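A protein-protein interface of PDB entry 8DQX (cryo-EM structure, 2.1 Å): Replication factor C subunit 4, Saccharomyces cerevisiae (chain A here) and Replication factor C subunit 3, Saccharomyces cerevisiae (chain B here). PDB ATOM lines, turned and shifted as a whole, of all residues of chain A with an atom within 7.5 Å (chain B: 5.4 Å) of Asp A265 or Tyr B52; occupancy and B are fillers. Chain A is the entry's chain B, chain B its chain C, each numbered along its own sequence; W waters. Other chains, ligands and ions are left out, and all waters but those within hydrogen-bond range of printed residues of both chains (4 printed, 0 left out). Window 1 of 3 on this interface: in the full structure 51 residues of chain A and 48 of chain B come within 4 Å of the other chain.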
ATOM      1  N   ASP A 229       2.514   0.009  27.126  1.00  0.00           N
ATOM      2  CA  ASP A 229       2.360   0.684  25.845  1.00  0.00           C
ATOM      3  C   ASP A 229       3.498   1.671  25.624  1.00  0.00           C
ATOM      4  O   ASP A 229       3.940   2.350  26.554  1.00  0.00           O
ATOM      5  CB  ASP A 229       1.023   1.428  25.785  1.00  0.00           C
ATOM      6  CG  ASP A 229      -0.148   0.514  25.464  1.00  0.00           C
ATOM      7  OD1 ASP A 229      -0.353   0.207  24.274  1.00  0.00           O
ATOM      8  OD2 ASP A 229      -0.869   0.112  26.402  1.00  0.00           O
ATOM      9  N   HIS A 232       2.074   7.190  23.811  1.00  0.00           N
ATOM     10  CA  HIS A 232       1.309   7.602  22.639  1.00  0.00           C
ATOM     11  C   HIS A 232       1.653   9.015  22.162  1.00  0.00           C
ATOM     12  O   HIS A 232       1.415   9.319  20.989  1.00  0.00           O
ATOM     13  CB  HIS A 232      -0.198   7.427  22.892  1.00  0.00           C
ATOM     14  CG  HIS A 232      -0.849   8.553  23.631  1.00  0.00           C
ATOM     15  ND1 HIS A 232      -0.788   8.673  25.003  1.00  0.00           N
ATOM     16  CD2 HIS A 232      -1.623   9.575  23.199  1.00  0.00           C
ATOM     17  CE1 HIS A 232      -1.468   9.741  25.378  1.00  0.00           C
ATOM     18  NE2 HIS A 232      -1.986  10.305  24.303  1.00  0.00           N
ATOM     19  N   VAL A 236       1.967   9.891  18.223  1.00  0.00           N
ATOM     20  CA  VAL A 236       1.314  11.048  17.618  1.00  0.00           C
ATOM     21  C   VAL A 236       2.331  11.914  16.887  1.00  0.00           C
ATOM     22  O   VAL A 236       2.053  12.446  15.808  1.00  0.00           O
ATOM     23  CB  VAL A 236       0.556  11.848  18.693  1.00  0.00           C
ATOM     24  CG1 VAL A 236       0.184  13.236  18.175  1.00  0.00           C
ATOM     25  CG2 VAL A 236      -0.683  11.087  19.135  1.00  0.00           C
ATOM     26  N   LEU A 256      -3.185   3.963  16.921  1.00  0.00           N
ATOM     27  CA  LEU A 256      -3.991   4.755  17.845  1.00  0.00           C
ATOM     28  C   LEU A 256      -5.454   4.335  17.850  1.00  0.00           C
ATOM     29  O   LEU A 256      -5.963   3.927  18.897  1.00  0.00           O
ATOM     30  CB  LEU A 256      -3.853   6.241  17.492  1.00  0.00           C
ATOM     31  CG  LEU A 256      -2.431   6.799  17.625  1.00  0.00           C
ATOM     32  CD1 LEU A 256      -2.357   8.186  16.996  1.00  0.00           C
ATOM     33  CD2 LEU A 256      -1.967   6.846  19.072  1.00  0.00           C
ATOM     34  N   LYS A 259      -6.183   0.647  18.768  1.00  0.00           N
ATOM     35  CA  LYS A 259      -5.751   0.288  20.112  1.00  0.00           C
ATOM     36  C   LYS A 259      -6.724   0.753  21.186  1.00  0.00           C
ATOM     37  O   LYS A 259      -6.559   0.377  22.350  1.00  0.00           O
ATOM     38  CB  LYS A 259      -4.367   0.874  20.408  1.00  0.00           C
ATOM     39  CG  LYS A 259      -3.314   0.522  19.385  1.00  0.00           C
ATOM     40  CD  LYS A 259      -3.001  -0.958  19.391  1.00  0.00           C
ATOM     41  CE  LYS A 259      -1.600  -1.224  18.874  1.00  0.00           C
ATOM     42  NZ  LYS A 259      -0.562  -0.629  19.755  1.00  0.00           N
ATOM     43  N   GLY A 260      -7.718   1.567  20.830  1.00  0.00           N
ATOM     44  CA  GLY A 260      -8.725   2.018  21.764  1.00  0.00           C
ATOM     45  C   GLY A 260      -8.538   3.419  22.312  1.00  0.00           C
ATOM     46  O   GLY A 260      -9.327   3.833  23.169  1.00  0.00           O
ATOM     47  N   TYR A 261      -7.527   4.158  21.857  1.00  0.00           N
ATOM     48  CA  TYR A 261      -7.370   5.541  22.288  1.00  0.00           C
ATOM     49  C   TYR A 261      -8.548   6.378  21.800  1.00  0.00           C
ATOM     50  O   TYR A 261      -8.946   6.289  20.637  1.00  0.00           O
ATOM     51  CB  TYR A 261      -6.053   6.113  21.763  1.00  0.00           C
ATOM     52  CG  TYR A 261      -4.832   5.536  22.434  1.00  0.00           C
ATOM     53  CD1 TYR A 261      -4.361   6.063  23.631  1.00  0.00           C
ATOM     54  CD2 TYR A 261      -4.151   4.461  21.879  1.00  0.00           C
ATOM     55  CE1 TYR A 261      -3.249   5.538  24.253  1.00  0.00           C
ATOM     56  CE2 TYR A 261      -3.029   3.931  22.492  1.00  0.00           C
ATOM     57  CZ  TYR A 261      -2.585   4.475  23.682  1.00  0.00           C
ATOM     58  OH  TYR A 261      -1.476   3.955  24.306  1.00  0.00           O
ATOM     59  N   SER A 262      -9.108   7.188  22.695  1.00  0.00           N
ATOM     60  CA  SER A 262     -10.271   7.995  22.349  1.00  0.00           C
ATOM     61  C   SER A 262      -9.885   9.114  21.381  1.00  0.00           C
ATOM     62  O   SER A 262      -8.736   9.552  21.316  1.00  0.00           O
ATOM     63  CB  SER A 262     -10.915   8.588  23.606  1.00  0.00           C
ATOM     64  OG  SER A 262     -10.005   9.393  24.336  1.00  0.00           O
ATOM     65  N   SER A 263     -10.877   9.572  20.615  1.00  0.00           N
ATOM     66  CA  SER A 263     -10.636  10.656  19.670  1.00  0.00           C
ATOM     67  C   SER A 263     -10.237  11.940  20.393  1.00  0.00           C
ATOM     68  O   SER A 263      -9.376  12.688  19.914  1.00  0.00           O
ATOM     69  CB  SER A 263     -11.874  10.868  18.792  1.00  0.00           C
ATOM     70  OG  SER A 263     -12.959  11.402  19.521  1.00  0.00           O
ATOM     71  N   ILE A 264     -10.831  12.203  21.560  1.00  0.00           N
ATOM     72  CA  ILE A 264     -10.470  13.398  22.323  1.00  0.00           C
ATOM     73  C   ILE A 264      -9.028  13.302  22.821  1.00  0.00           C
ATOM     74  O   ILE A 264      -8.282  14.291  22.801  1.00  0.00           O
ATOM     75  CB  ILE A 264     -11.470  13.615  23.478  1.00  0.00           C
ATOM     76  CG1 ILE A 264     -11.281  15.000  24.106  1.00  0.00           C
ATOM     77  CG2 ILE A 264     -11.320  12.537  24.540  1.00  0.00           C
ATOM     78  CD1 ILE A 264     -11.830  16.133  23.272  1.00  0.00           C
ATOM     79  N   ASP A 265      -8.608  12.113  23.261  1.00  0.00           N
ATOM     80  CA  ASP A 265      -7.215  11.935  23.670  1.00  0.00           C
ATOM     81  C   ASP A 265      -6.268  12.170  22.498  1.00  0.00           C
ATOM     82  O   ASP A 265      -5.260  12.877  22.634  1.00  0.00           O
ATOM     83  CB  ASP A 265      -7.006  10.534  24.253  1.00  0.00           C
ATOM     84  CG  ASP A 265      -7.374  10.445  25.732  1.00  0.00           C
ATOM     85  OD1 ASP A 265      -7.258  11.456  26.450  1.00  0.00           O
ATOM     86  OD2 ASP A 265      -7.777   9.355  26.179  1.00  0.00           O
ATOM     87  N   ILE A 266      -6.596  11.613  21.329  1.00  0.00           N
ATOM     88  CA  ILE A 266      -5.750  11.779  20.150  1.00  0.00           C
ATOM     89  C   ILE A 266      -5.626  13.254  19.784  1.00  0.00           C
ATOM     90  O   ILE A 266      -4.529  13.749  19.511  1.00  0.00           O
ATOM     91  CB  ILE A 266      -6.297  10.945  18.976  1.00  0.00           C
ATOM     92  CG1 ILE A 266      -6.212   9.450  19.303  1.00  0.00           C
ATOM     93  CG2 ILE A 266      -5.536  11.260  17.684  1.00  0.00           C
ATOM     94  CD1 ILE A 266      -7.013   8.560  18.375  1.00  0.00           C
ATOM     95  N   VAL A 267      -6.747  13.984  19.786  1.00  0.00           N
ATOM     96  CA  VAL A 267      -6.713  15.373  19.327  1.00  0.00           C
ATOM     97  C   VAL A 267      -5.984  16.267  20.333  1.00  0.00           C
ATOM     98  O   VAL A 267      -5.195  17.141  19.944  1.00  0.00           O
ATOM     99  CB  VAL A 267      -8.138  15.881  19.023  1.00  0.00           C
ATOM    100  CG1 VAL A 267      -8.876  16.293  20.292  1.00  0.00           C
ATOM    101  CG2 VAL A 267      -8.089  17.042  18.032  1.00  0.00           C
ATOM    102  N   THR A 268      -6.223  16.069  21.635  1.00  0.00           N
ATOM    103  CA  THR A 268      -5.520  16.888  22.622  1.00  0.00           C
ATOM    104  C   THR A 268      -4.018  16.611  22.598  1.00  0.00           C
ATOM    105  O   THR A 268      -3.205  17.542  22.694  1.00  0.00           O
ATOM    106  CB  THR A 268      -6.099  16.663  24.022  1.00  0.00           C
ATOM    107  OG1 THR A 268      -6.127  15.263  24.327  1.00  0.00           O
ATOM    108  CG2 THR A 268      -7.517  17.229  24.112  1.00  0.00           C
ATOM    109  N   THR A 269      -3.626  15.343  22.440  1.00  0.00           N
ATOM    110  CA  THR A 269      -2.208  15.038  22.311  1.00  0.00           C
ATOM    111  C   THR A 269      -1.625  15.657  21.047  1.00  0.00           C
ATOM    112  O   THR A 269      -0.485  16.129  21.053  1.00  0.00           O
ATOM    113  CB  THR A 269      -1.985  13.525  22.316  1.00  0.00           C
ATOM    114  OG1 THR A 269      -2.426  12.984  23.567  1.00  0.00           O
ATOM    115  CG2 THR A 269      -0.505  13.201  22.119  1.00  0.00           C
ATOM    116  N   SER A 270      -2.382  15.645  19.945  1.00  0.00           N
ATOM    117  CA  SER A 270      -1.908  16.280  18.722  1.00  0.00           C
ATOM    118  C   SER A 270      -1.623  17.759  18.950  1.00  0.00           C
ATOM    119  O   SER A 270      -0.594  18.277  18.503  1.00  0.00           O
ATOM    120  CB  SER A 270      -2.934  16.101  17.602  1.00  0.00           C
ATOM    121  OG  SER A 270      -2.959  14.765  17.136  1.00  0.00           O
ATOM    122  N   PHE A 271      -2.529  18.454  19.641  1.00  0.00           N
ATOM    123  CA  PHE A 271      -2.297  19.861  19.961  1.00  0.00           C
ATOM    124  C   PHE A 271      -1.025  20.035  20.786  1.00  0.00           C
ATOM    125  O   PHE A 271      -0.163  20.865  20.462  1.00  0.00           O
ATOM    126  CB  PHE A 271      -3.503  20.434  20.708  1.00  0.00           C
ATOM    127  CG  PHE A 271      -3.392  21.905  21.030  1.00  0.00           C
ATOM    128  CD1 PHE A 271      -2.526  22.362  22.015  1.00  0.00           C
ATOM    129  CD2 PHE A 271      -4.170  22.834  20.352  1.00  0.00           C
ATOM    130  CE1 PHE A 271      -2.431  23.711  22.309  1.00  0.00           C
ATOM    131  CE2 PHE A 271      -4.083  24.186  20.649  1.00  0.00           C
ATOM    132  CZ  PHE A 271      -3.215  24.623  21.626  1.00  0.00           C
ATOM    133  N   ILE A 299     -15.250  17.413  17.787  1.00  0.00           N
ATOM    134  CA  ILE A 299     -15.317  16.250  18.666  1.00  0.00           C
ATOM    135  C   ILE A 299     -16.080  16.586  19.941  1.00  0.00           C
ATOM    136  O   ILE A 299     -16.912  15.800  20.405  1.00  0.00           O
ATOM    137  CB  ILE A 299     -13.903  15.718  18.972  1.00  0.00           C
ATOM    138  CG1 ILE A 299     -13.238  15.218  17.688  1.00  0.00           C
ATOM    139  CG2 ILE A 299     -13.958  14.615  20.023  1.00  0.00           C
ATOM    140  CD1 ILE A 299     -11.790  14.844  17.856  1.00  0.00           C
ATOM    141  N   LEU A 309     -10.857  12.674  12.379  1.00  0.00           N
ATOM    142  CA  LEU A 309      -9.409  12.658  12.581  1.00  0.00           C
ATOM    143  C   LEU A 309      -8.663  12.501  11.257  1.00  0.00           C
ATOM    144  O   LEU A 309      -7.631  13.150  11.034  1.00  0.00           O
ATOM    145  CB  LEU A 309      -9.039  11.538  13.553  1.00  0.00           C
ATOM    146  CG  LEU A 309      -9.547  11.692  14.995  1.00  0.00           C
ATOM    147  CD1 LEU A 309      -9.348  10.399  15.778  1.00  0.00           C
ATOM    148  CD2 LEU A 309      -8.858  12.844  15.698  1.00  0.00           C
ATOM    149  N   LEU B  50      -4.868   1.380  37.154  1.00  0.00           N
ATOM    150  CA  LEU B  50      -5.655   2.188  36.234  1.00  0.00           C
ATOM    151  C   LEU B  50      -6.082   1.301  35.074  1.00  0.00           C
ATOM    152  O   LEU B  50      -5.240   0.668  34.433  1.00  0.00           O
ATOM    153  CB  LEU B  50      -4.865   3.404  35.720  1.00  0.00           C
ATOM    154  CG  LEU B  50      -5.463   4.157  34.521  1.00  0.00           C
ATOM    155  CD1 LEU B  50      -6.661   4.990  34.956  1.00  0.00           C
ATOM    156  CD2 LEU B  50      -4.419   5.038  33.844  1.00  0.00           C
ATOM    157  N   PHE B  51      -7.384   1.237  34.821  1.00  0.00           N
ATOM    158  CA  PHE B  51      -7.942   0.543  33.665  1.00  0.00           C
ATOM    159  C   PHE B  51      -8.422   1.608  32.683  1.00  0.00           C
ATOM    160  O   PHE B  51      -9.368   2.348  32.975  1.00  0.00           O
ATOM    161  CB  PHE B  51      -9.086  -0.393  34.064  1.00  0.00           C
ATOM    162  CG  PHE B  51      -8.661  -1.604  34.871  1.00  0.00           C
ATOM    163  CD1 PHE B  51      -7.323  -1.941  35.022  1.00  0.00           C
ATOM    164  CD2 PHE B  51      -9.618  -2.421  35.455  1.00  0.00           C
ATOM    165  CE1 PHE B  51      -6.951  -3.063  35.754  1.00  0.00           C
ATOM    166  CE2 PHE B  51      -9.253  -3.540  36.188  1.00  0.00           C
ATOM    167  CZ  PHE B  51      -7.915  -3.862  36.335  1.00  0.00           C
ATOM    168  N   TYR B  52      -7.778   1.676  31.521  1.00  0.00           N
ATOM    169  CA  TYR B  52      -8.090   2.673  30.504  1.00  0.00           C
ATOM    170  C   TYR B  52      -8.594   1.974  29.255  1.00  0.00           C
ATOM    171  O   TYR B  52      -7.946   1.045  28.768  1.00  0.00           O
ATOM    172  CB  TYR B  52      -6.859   3.516  30.158  1.00  0.00           C
ATOM    173  CG  TYR B  52      -7.027   4.360  28.911  1.00  0.00           C
ATOM    174  CD1 TYR B  52      -7.719   5.563  28.954  1.00  0.00           C
ATOM    175  CD2 TYR B  52      -6.504   3.950  27.690  1.00  0.00           C
ATOM    176  CE1 TYR B  52      -7.880   6.340  27.827  1.00  0.00           C
ATOM    177  CE2 TYR B  52      -6.661   4.725  26.547  1.00  0.00           C
ATOM    178  CZ  TYR B  52      -7.350   5.922  26.625  1.00  0.00           C
ATOM    179  OH  TYR B  52      -7.516   6.705  25.508  1.00  0.00           O
ATOM    180  N   GLY B  53      -9.725   2.424  28.718  1.00  0.00           N
ATOM    181  CA  GLY B  53     -10.205   1.829  27.487  1.00  0.00           C
ATOM    182  C   GLY B  53     -11.542   2.330  26.976  1.00  0.00           C
ATOM    183  O   GLY B  53     -12.261   3.071  27.650  1.00  0.00           O
ATOM    184  N   PRO B  54     -11.897   1.917  25.758  1.00  0.00           N
ATOM    185  CA  PRO B  54     -13.159   2.369  25.146  1.00  0.00           C
ATOM    186  C   PRO B  54     -14.362   1.637  25.717  1.00  0.00           C
ATOM    187  O   PRO B  54     -14.215   0.631  26.425  1.00  0.00           O
ATOM    188  CB  PRO B  54     -12.967   2.051  23.655  1.00  0.00           C
ATOM    189  CG  PRO B  54     -11.905   1.023  23.591  1.00  0.00           C
ATOM    190  CD  PRO B  54     -11.060   1.143  24.824  1.00  0.00           C
ATOM    191  N   LYS B  59     -13.952  -3.210  31.644  1.00  0.00           N
ATOM    192  CA  LYS B  59     -13.211  -2.615  32.755  1.00  0.00           C
ATOM    193  C   LYS B  59     -13.946  -2.800  34.085  1.00  0.00           C
ATOM    194  O   LYS B  59     -13.399  -3.370  35.040  1.00  0.00           O
ATOM    195  CB  LYS B  59     -12.954  -1.134  32.460  1.00  0.00           C
ATOM    196  CG  LYS B  59     -12.130  -0.901  31.191  1.00  0.00           C
ATOM    197  CD  LYS B  59     -11.745   0.566  30.994  1.00  0.00           C
ATOM    198  CE  LYS B  59     -12.953   1.449  30.693  1.00  0.00           C
ATOM    199  NZ  LYS B  59     -13.778   0.935  29.570  1.00  0.00           N
ATOM    200  N   ALA B 147     -11.180   4.600  33.447  1.00  0.00           N
ATOM    201  CA  ALA B 147     -11.414   5.760  32.593  1.00  0.00           C
ATOM    202  C   ALA B 147     -11.519   5.381  31.117  1.00  0.00           C
ATOM    203  O   ALA B 147     -10.908   4.409  30.650  1.00  0.00           O
ATOM    204  CB  ALA B 147     -10.307   6.801  32.773  1.00  0.00           C
ATOM    205  N   ASN B 148     -12.301   6.191  30.394  1.00  0.00           N
ATOM    206  CA  ASN B 148     -12.324   6.197  28.937  1.00  0.00           C
ATOM    207  C   ASN B 148     -11.464   7.299  28.332  1.00  0.00           C
ATOM    208  O   ASN B 148     -11.085   7.194  27.163  1.00  0.00           O
ATOM    209  CB  ASN B 148     -13.756   6.381  28.416  1.00  0.00           C
ATOM    210  CG  ASN B 148     -14.709   5.313  28.908  1.00  0.00           C
ATOM    211  OD1 ASN B 148     -15.679   5.613  29.589  1.00  0.00           O
ATOM    212  ND2 ASN B 148     -14.442   4.066  28.552  1.00  0.00           N
ATOM    213  N   TYR B 149     -11.154   8.352  29.087  1.00  0.00           N
ATOM    214  CA  TYR B 149     -10.481   9.534  28.555  1.00  0.00           C
ATOM    215  C   TYR B 149      -9.329   9.912  29.477  1.00  0.00           C
ATOM    216  O   TYR B 149      -9.551  10.462  30.559  1.00  0.00           O
ATOM    217  CB  TYR B 149     -11.464  10.694  28.409  1.00  0.00           C
ATOM    218  CG  TYR B 149     -12.779  10.311  27.761  1.00  0.00           C
ATOM    219  CD1 TYR B 149     -12.828   9.888  26.438  1.00  0.00           C
ATOM    220  CD2 TYR B 149     -13.968  10.375  28.472  1.00  0.00           C
ATOM    221  CE1 TYR B 149     -14.026   9.542  25.844  1.00  0.00           C
ATOM    222  CE2 TYR B 149     -15.172  10.026  27.889  1.00  0.00           C
ATOM    223  CZ  TYR B 149     -15.198   9.611  26.579  1.00  0.00           C
ATOM    224  OH  TYR B 149     -16.397   9.268  26.003  1.00  0.00           O
ATOM    225  N   ALA B 150      -8.100   9.627  29.044  1.00  0.00           N
ATOM    226  CA  ALA B 150      -6.938   9.908  29.880  1.00  0.00           C
ATOM    227  C   ALA B 150      -6.696  11.405  30.049  1.00  0.00           C
ATOM    228  O   ALA B 150      -6.118  11.822  31.058  1.00  0.00           O
ATOM    229  CB  ALA B 150      -5.697   9.240  29.291  1.00  0.00           C
ATOM    230  N   HIS B 151      -7.126  12.225  29.087  1.00  0.00           N
ATOM    231  CA  HIS B 151      -6.781  13.643  29.115  1.00  0.00           C
ATOM    232  C   HIS B 151      -7.430  14.394  30.273  1.00  0.00           C
ATOM    233  O   HIS B 151      -6.936  15.462  30.645  1.00  0.00           O
ATOM    234  CB  HIS B 151      -7.155  14.309  27.786  1.00  0.00           C
ATOM    235  CG  HIS B 151      -8.604  14.664  27.667  1.00  0.00           C
ATOM    236  ND1 HIS B 151      -9.074  15.949  27.837  1.00  0.00           N
ATOM    237  CD2 HIS B 151      -9.687  13.904  27.377  1.00  0.00           C
ATOM    238  CE1 HIS B 151     -10.384  15.964  27.664  1.00  0.00           C
ATOM    239  NE2 HIS B 151     -10.781  14.735  27.383  1.00  0.00           N
ATOM    240  N   LYS B 152      -8.507  13.876  30.853  1.00  0.00           N
ATOM    241  CA  LYS B 152      -9.111  14.510  32.020  1.00  0.00           C
ATOM    242  C   LYS B 152      -8.479  14.058  33.331  1.00  0.00           C
ATOM    243  O   LYS B 152      -8.849  14.576  34.389  1.00  0.00           O
ATOM    244  CB  LYS B 152     -10.626  14.255  32.062  1.00  0.00           C
ATOM    245  CG  LYS B 152     -11.346  14.326  30.721  1.00  0.00           C
ATOM    246  CD  LYS B 152     -12.558  13.417  30.710  1.00  0.00           C
ATOM    247  CE  LYS B 152     -13.564  13.786  29.628  1.00  0.00           C
ATOM    248  NZ  LYS B 152     -14.931  13.960  30.193  1.00  0.00           N
ATOM    249  N   ARG B 163      -0.739   1.286  34.835  1.00  0.00           N
ATOM    250  CA  ARG B 163      -1.693   1.432  33.742  1.00  0.00           C
ATOM    251  C   ARG B 163      -1.901   0.115  33.004  1.00  0.00           C
ATOM    252  O   ARG B 163      -0.952  -0.633  32.761  1.00  0.00           O
ATOM    253  CB  ARG B 163      -1.218   2.509  32.767  1.00  0.00           C
ATOM    254  CG  ARG B 163      -1.956   2.540  31.433  1.00  0.00           C
ATOM    255  CD  ARG B 163      -1.512   3.736  30.605  1.00  0.00           C
ATOM    256  NE  ARG B 163      -2.343   3.959  29.428  1.00  0.00           N
ATOM    257  CZ  ARG B 163      -2.177   3.342  28.265  1.00  0.00           C
ATOM    258  NH1 ARG B 163      -1.278   2.383  28.115  1.00  0.00           N
ATOM    259  NH2 ARG B 163      -2.934   3.690  27.230  1.00  0.00           N
ATOM    260  N   PHE B 164      -3.155  -0.159  32.652  1.00  0.00           N
ATOM    261  CA  PHE B 164      -3.539  -1.309  31.846  1.00  0.00           C
ATOM    262  C   PHE B 164      -4.573  -0.861  30.825  1.00  0.00           C
ATOM    263  O   PHE B 164      -5.639  -0.352  31.195  1.00  0.00           O
ATOM    264  CB  PHE B 164      -4.116  -2.435  32.705  1.00  0.00           C
ATOM    265  CG  PHE B 164      -3.096  -3.144  33.543  1.00  0.00           C
ATOM    266  CD1 PHE B 164      -2.328  -4.160  33.009  1.00  0.00           C
ATOM    267  CD2 PHE B 164      -2.908  -2.793  34.864  1.00  0.00           C
ATOM    268  CE1 PHE B 164      -1.390  -4.813  33.779  1.00  0.00           C
ATOM    269  CE2 PHE B 164      -1.967  -3.441  35.639  1.00  0.00           C
ATOM    270  CZ  PHE B 164      -1.209  -4.450  35.098  1.00  0.00           C
ATOM    271  N   ARG B 165      -4.264  -1.061  29.550  1.00  0.00           N
ATOM    272  CA  ARG B 165      -5.142  -0.666  28.458  1.00  0.00           C
ATOM    273  C   ARG B 165      -6.009  -1.852  28.053  1.00  0.00           C
ATOM    274  O   ARG B 165      -5.490  -2.917  27.711  1.00  0.00           O
ATOM    275  CB  ARG B 165      -4.339  -0.164  27.260  1.00  0.00           C
ATOM    276  CG  ARG B 165      -5.198   0.177  26.050  1.00  0.00           C
ATOM    277  CD  ARG B 165      -4.370   0.777  24.933  1.00  0.00           C
ATOM    278  NE  ARG B 165      -3.301  -0.122  24.523  1.00  0.00           N
ATOM    279  CZ  ARG B 165      -3.468  -1.173  23.733  1.00  0.00           C
ATOM    280  NH1 ARG B 165      -4.650  -1.475  23.221  1.00  0.00           N
ATOM    281  NH2 ARG B 165      -2.423  -1.946  23.454  1.00  0.00           N
ATOM    282  N   PHE B 166      -7.321  -1.659  28.093  1.00  0.00           N
ATOM    283  CA  PHE B 166      -8.278  -2.628  27.577  1.00  0.00           C
ATOM    284  C   PHE B 166      -8.497  -2.345  26.096  1.00  0.00           C
ATOM    285  O   PHE B 166      -8.940  -1.253  25.727  1.00  0.00           O
ATOM    286  CB  PHE B 166      -9.596  -2.548  28.343  1.00  0.00           C
ATOM    287  CG  PHE B 166      -9.559  -3.215  29.682  1.00  0.00           C
ATOM    288  CD1 PHE B 166      -8.724  -2.743  30.685  1.00  0.00           C
ATOM    289  CD2 PHE B 166     -10.363  -4.310  29.945  1.00  0.00           C
ATOM    290  CE1 PHE B 166      -8.689  -3.354  31.916  1.00  0.00           C
ATOM    291  CE2 PHE B 166     -10.330  -4.925  31.180  1.00  0.00           C
ATOM    292  CZ  PHE B 166      -9.493  -4.448  32.166  1.00  0.00           C
HETATM  293  O   HOH W   1       0.780   0.602  29.906  1.00  0.00           O
HETATM  294  O   HOH W   2      -1.047  -1.003  28.920  1.00  0.00           O
HETATM  295  O   HOH W   3     -10.809   5.201  25.069  1.00  0.00           O
HETATM  296  O   HOH W   4      -4.775   8.252  26.374  1.00  0.00           O
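OD1 of Asp A265 is in hydrogen-bond range of N of His B151 (2.8 Å). The guanidinium group (NH1) of Arg B163 is in salt-bridge range of the side-chain carboxylate (OD2) of Asp A229 (2.9 Å). N of Ser A262 lies within hydrogen-bond range of OH of Tyr B52 (3.3 Å). The side-chain hydroxyl (OH) of Tyr A261 lies within hydrogen-bond range of the guanidinium group (NH2) of Arg B163 (3.3 Å). O of Lys A259 is in hydrogen-bond range of NH1 of Arg B165 (2.8 Å). OD2 of Asp A265 sits at hydrogen-bond distance from OH of Tyr B52, 2.7 Å away. The backbone NH (N) of Ala B150 is in hydrogen-bond range of the side-chain carboxylate (OD2) of Asp A265 (2.9 Å). The side-chain carboxylate (OD1) of Asp A229 is in salt-bridge range of the guanidinium group (NE) of Arg B165 (3.0 Å).
Printed residues of chain A within 4 Å of Arg B163: Asp A229 (2.9 Å) and Tyr A261 (3.3 Å). Of the printed residues of chain A, Arg B165 touches Asp A229 and Lys A259. The nearest residue of chain B that does not touch Asp A265 is Asn B148 (4.1 Å). The nearest residue of chain A that does not touch Tyr B52 is Gly A260 (4.1 Å).
Water W2 lies within hydrogen-bond range of the side-chain carboxylate (OD2) of Asp A229 (2.8 Å), the backbone NH (N) of Arg B165 (3.3 Å) and the guanidinium group (NH1) of Arg B163 (3.5 Å). Water W3 bridges the backbone carbonyl oxygen (O) of Gly A260 (2.8 Å) and the backbone carbonyl oxygen (O) of Asn B148 (2.9 Å). Water W4 lies within hydrogen-bond range of OD2 of Asp A265 (3.2 Å) and OH of Tyr B52 (3.3 Å). Water W1 bridges the guanidinium group of Arg B163 and the backbone NH of Asp A229.
Of the 19 printed residues of chain A, 8 touch a printed residue of chain B. Printed residues of chain A that touch a printed residue of chain B: Asp A229, Lys A259, Gly A260, Tyr A261, Ser A262, Ile A264, Asp A265 and Thr A268. Among the printed residues, 16 pairs touch across the chains. Among the printed residues, Asp or Glu carboxylates within 4 Å of a Lys or Arg side-chain nitrogen of the other chain: Asp A229 with Arg B163 and Asp A229 with Arg B165.
Among the printed residues, merely in contact across the chains: Gly A260 with Pro B54 (3.6 Å), Tyr A261 with Tyr B52 (3.4 Å), Ser A262 with Asn B148 (3.7 Å), Ser A262 with Tyr B149 (3.6 Å), Ile A264 with Tyr B149 (3.6 Å), Ile A264 with His B151 (3.3 Å), Asp A265 with Tyr B149 (3.6 Å) and Thr A268 with His B151 (3.7 Å).
The side-chain amino group (NZ) of Lys B59 sits close to the side-chain amide nitrogen (ND2) of Asn B148 (3.4 Å). NZ of Lys B59 lies within hydrogen-bond range of O of Pro B54 (3.2 Å). The backbone carbonyl oxygen of Asp A265 sits at hydrogen-bond distance from the side-chain hydroxyl of Thr A269 (3.0 Å). The backbone NH (N) of Tyr B52 lies within hydrogen-bond range of the backbone carbonyl oxygen (O) of Phe B164 (3.0 Å). The backbone carbonyl oxygen of Tyr B52 is in hydrogen-bond range of the backbone NH of Phe B166, 2.9 Å away. The backbone carbonyl oxygen (O) of Asp A265 lies within hydrogen-bond range of the side-chain hydroxyl (OG1) of Thr A268.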
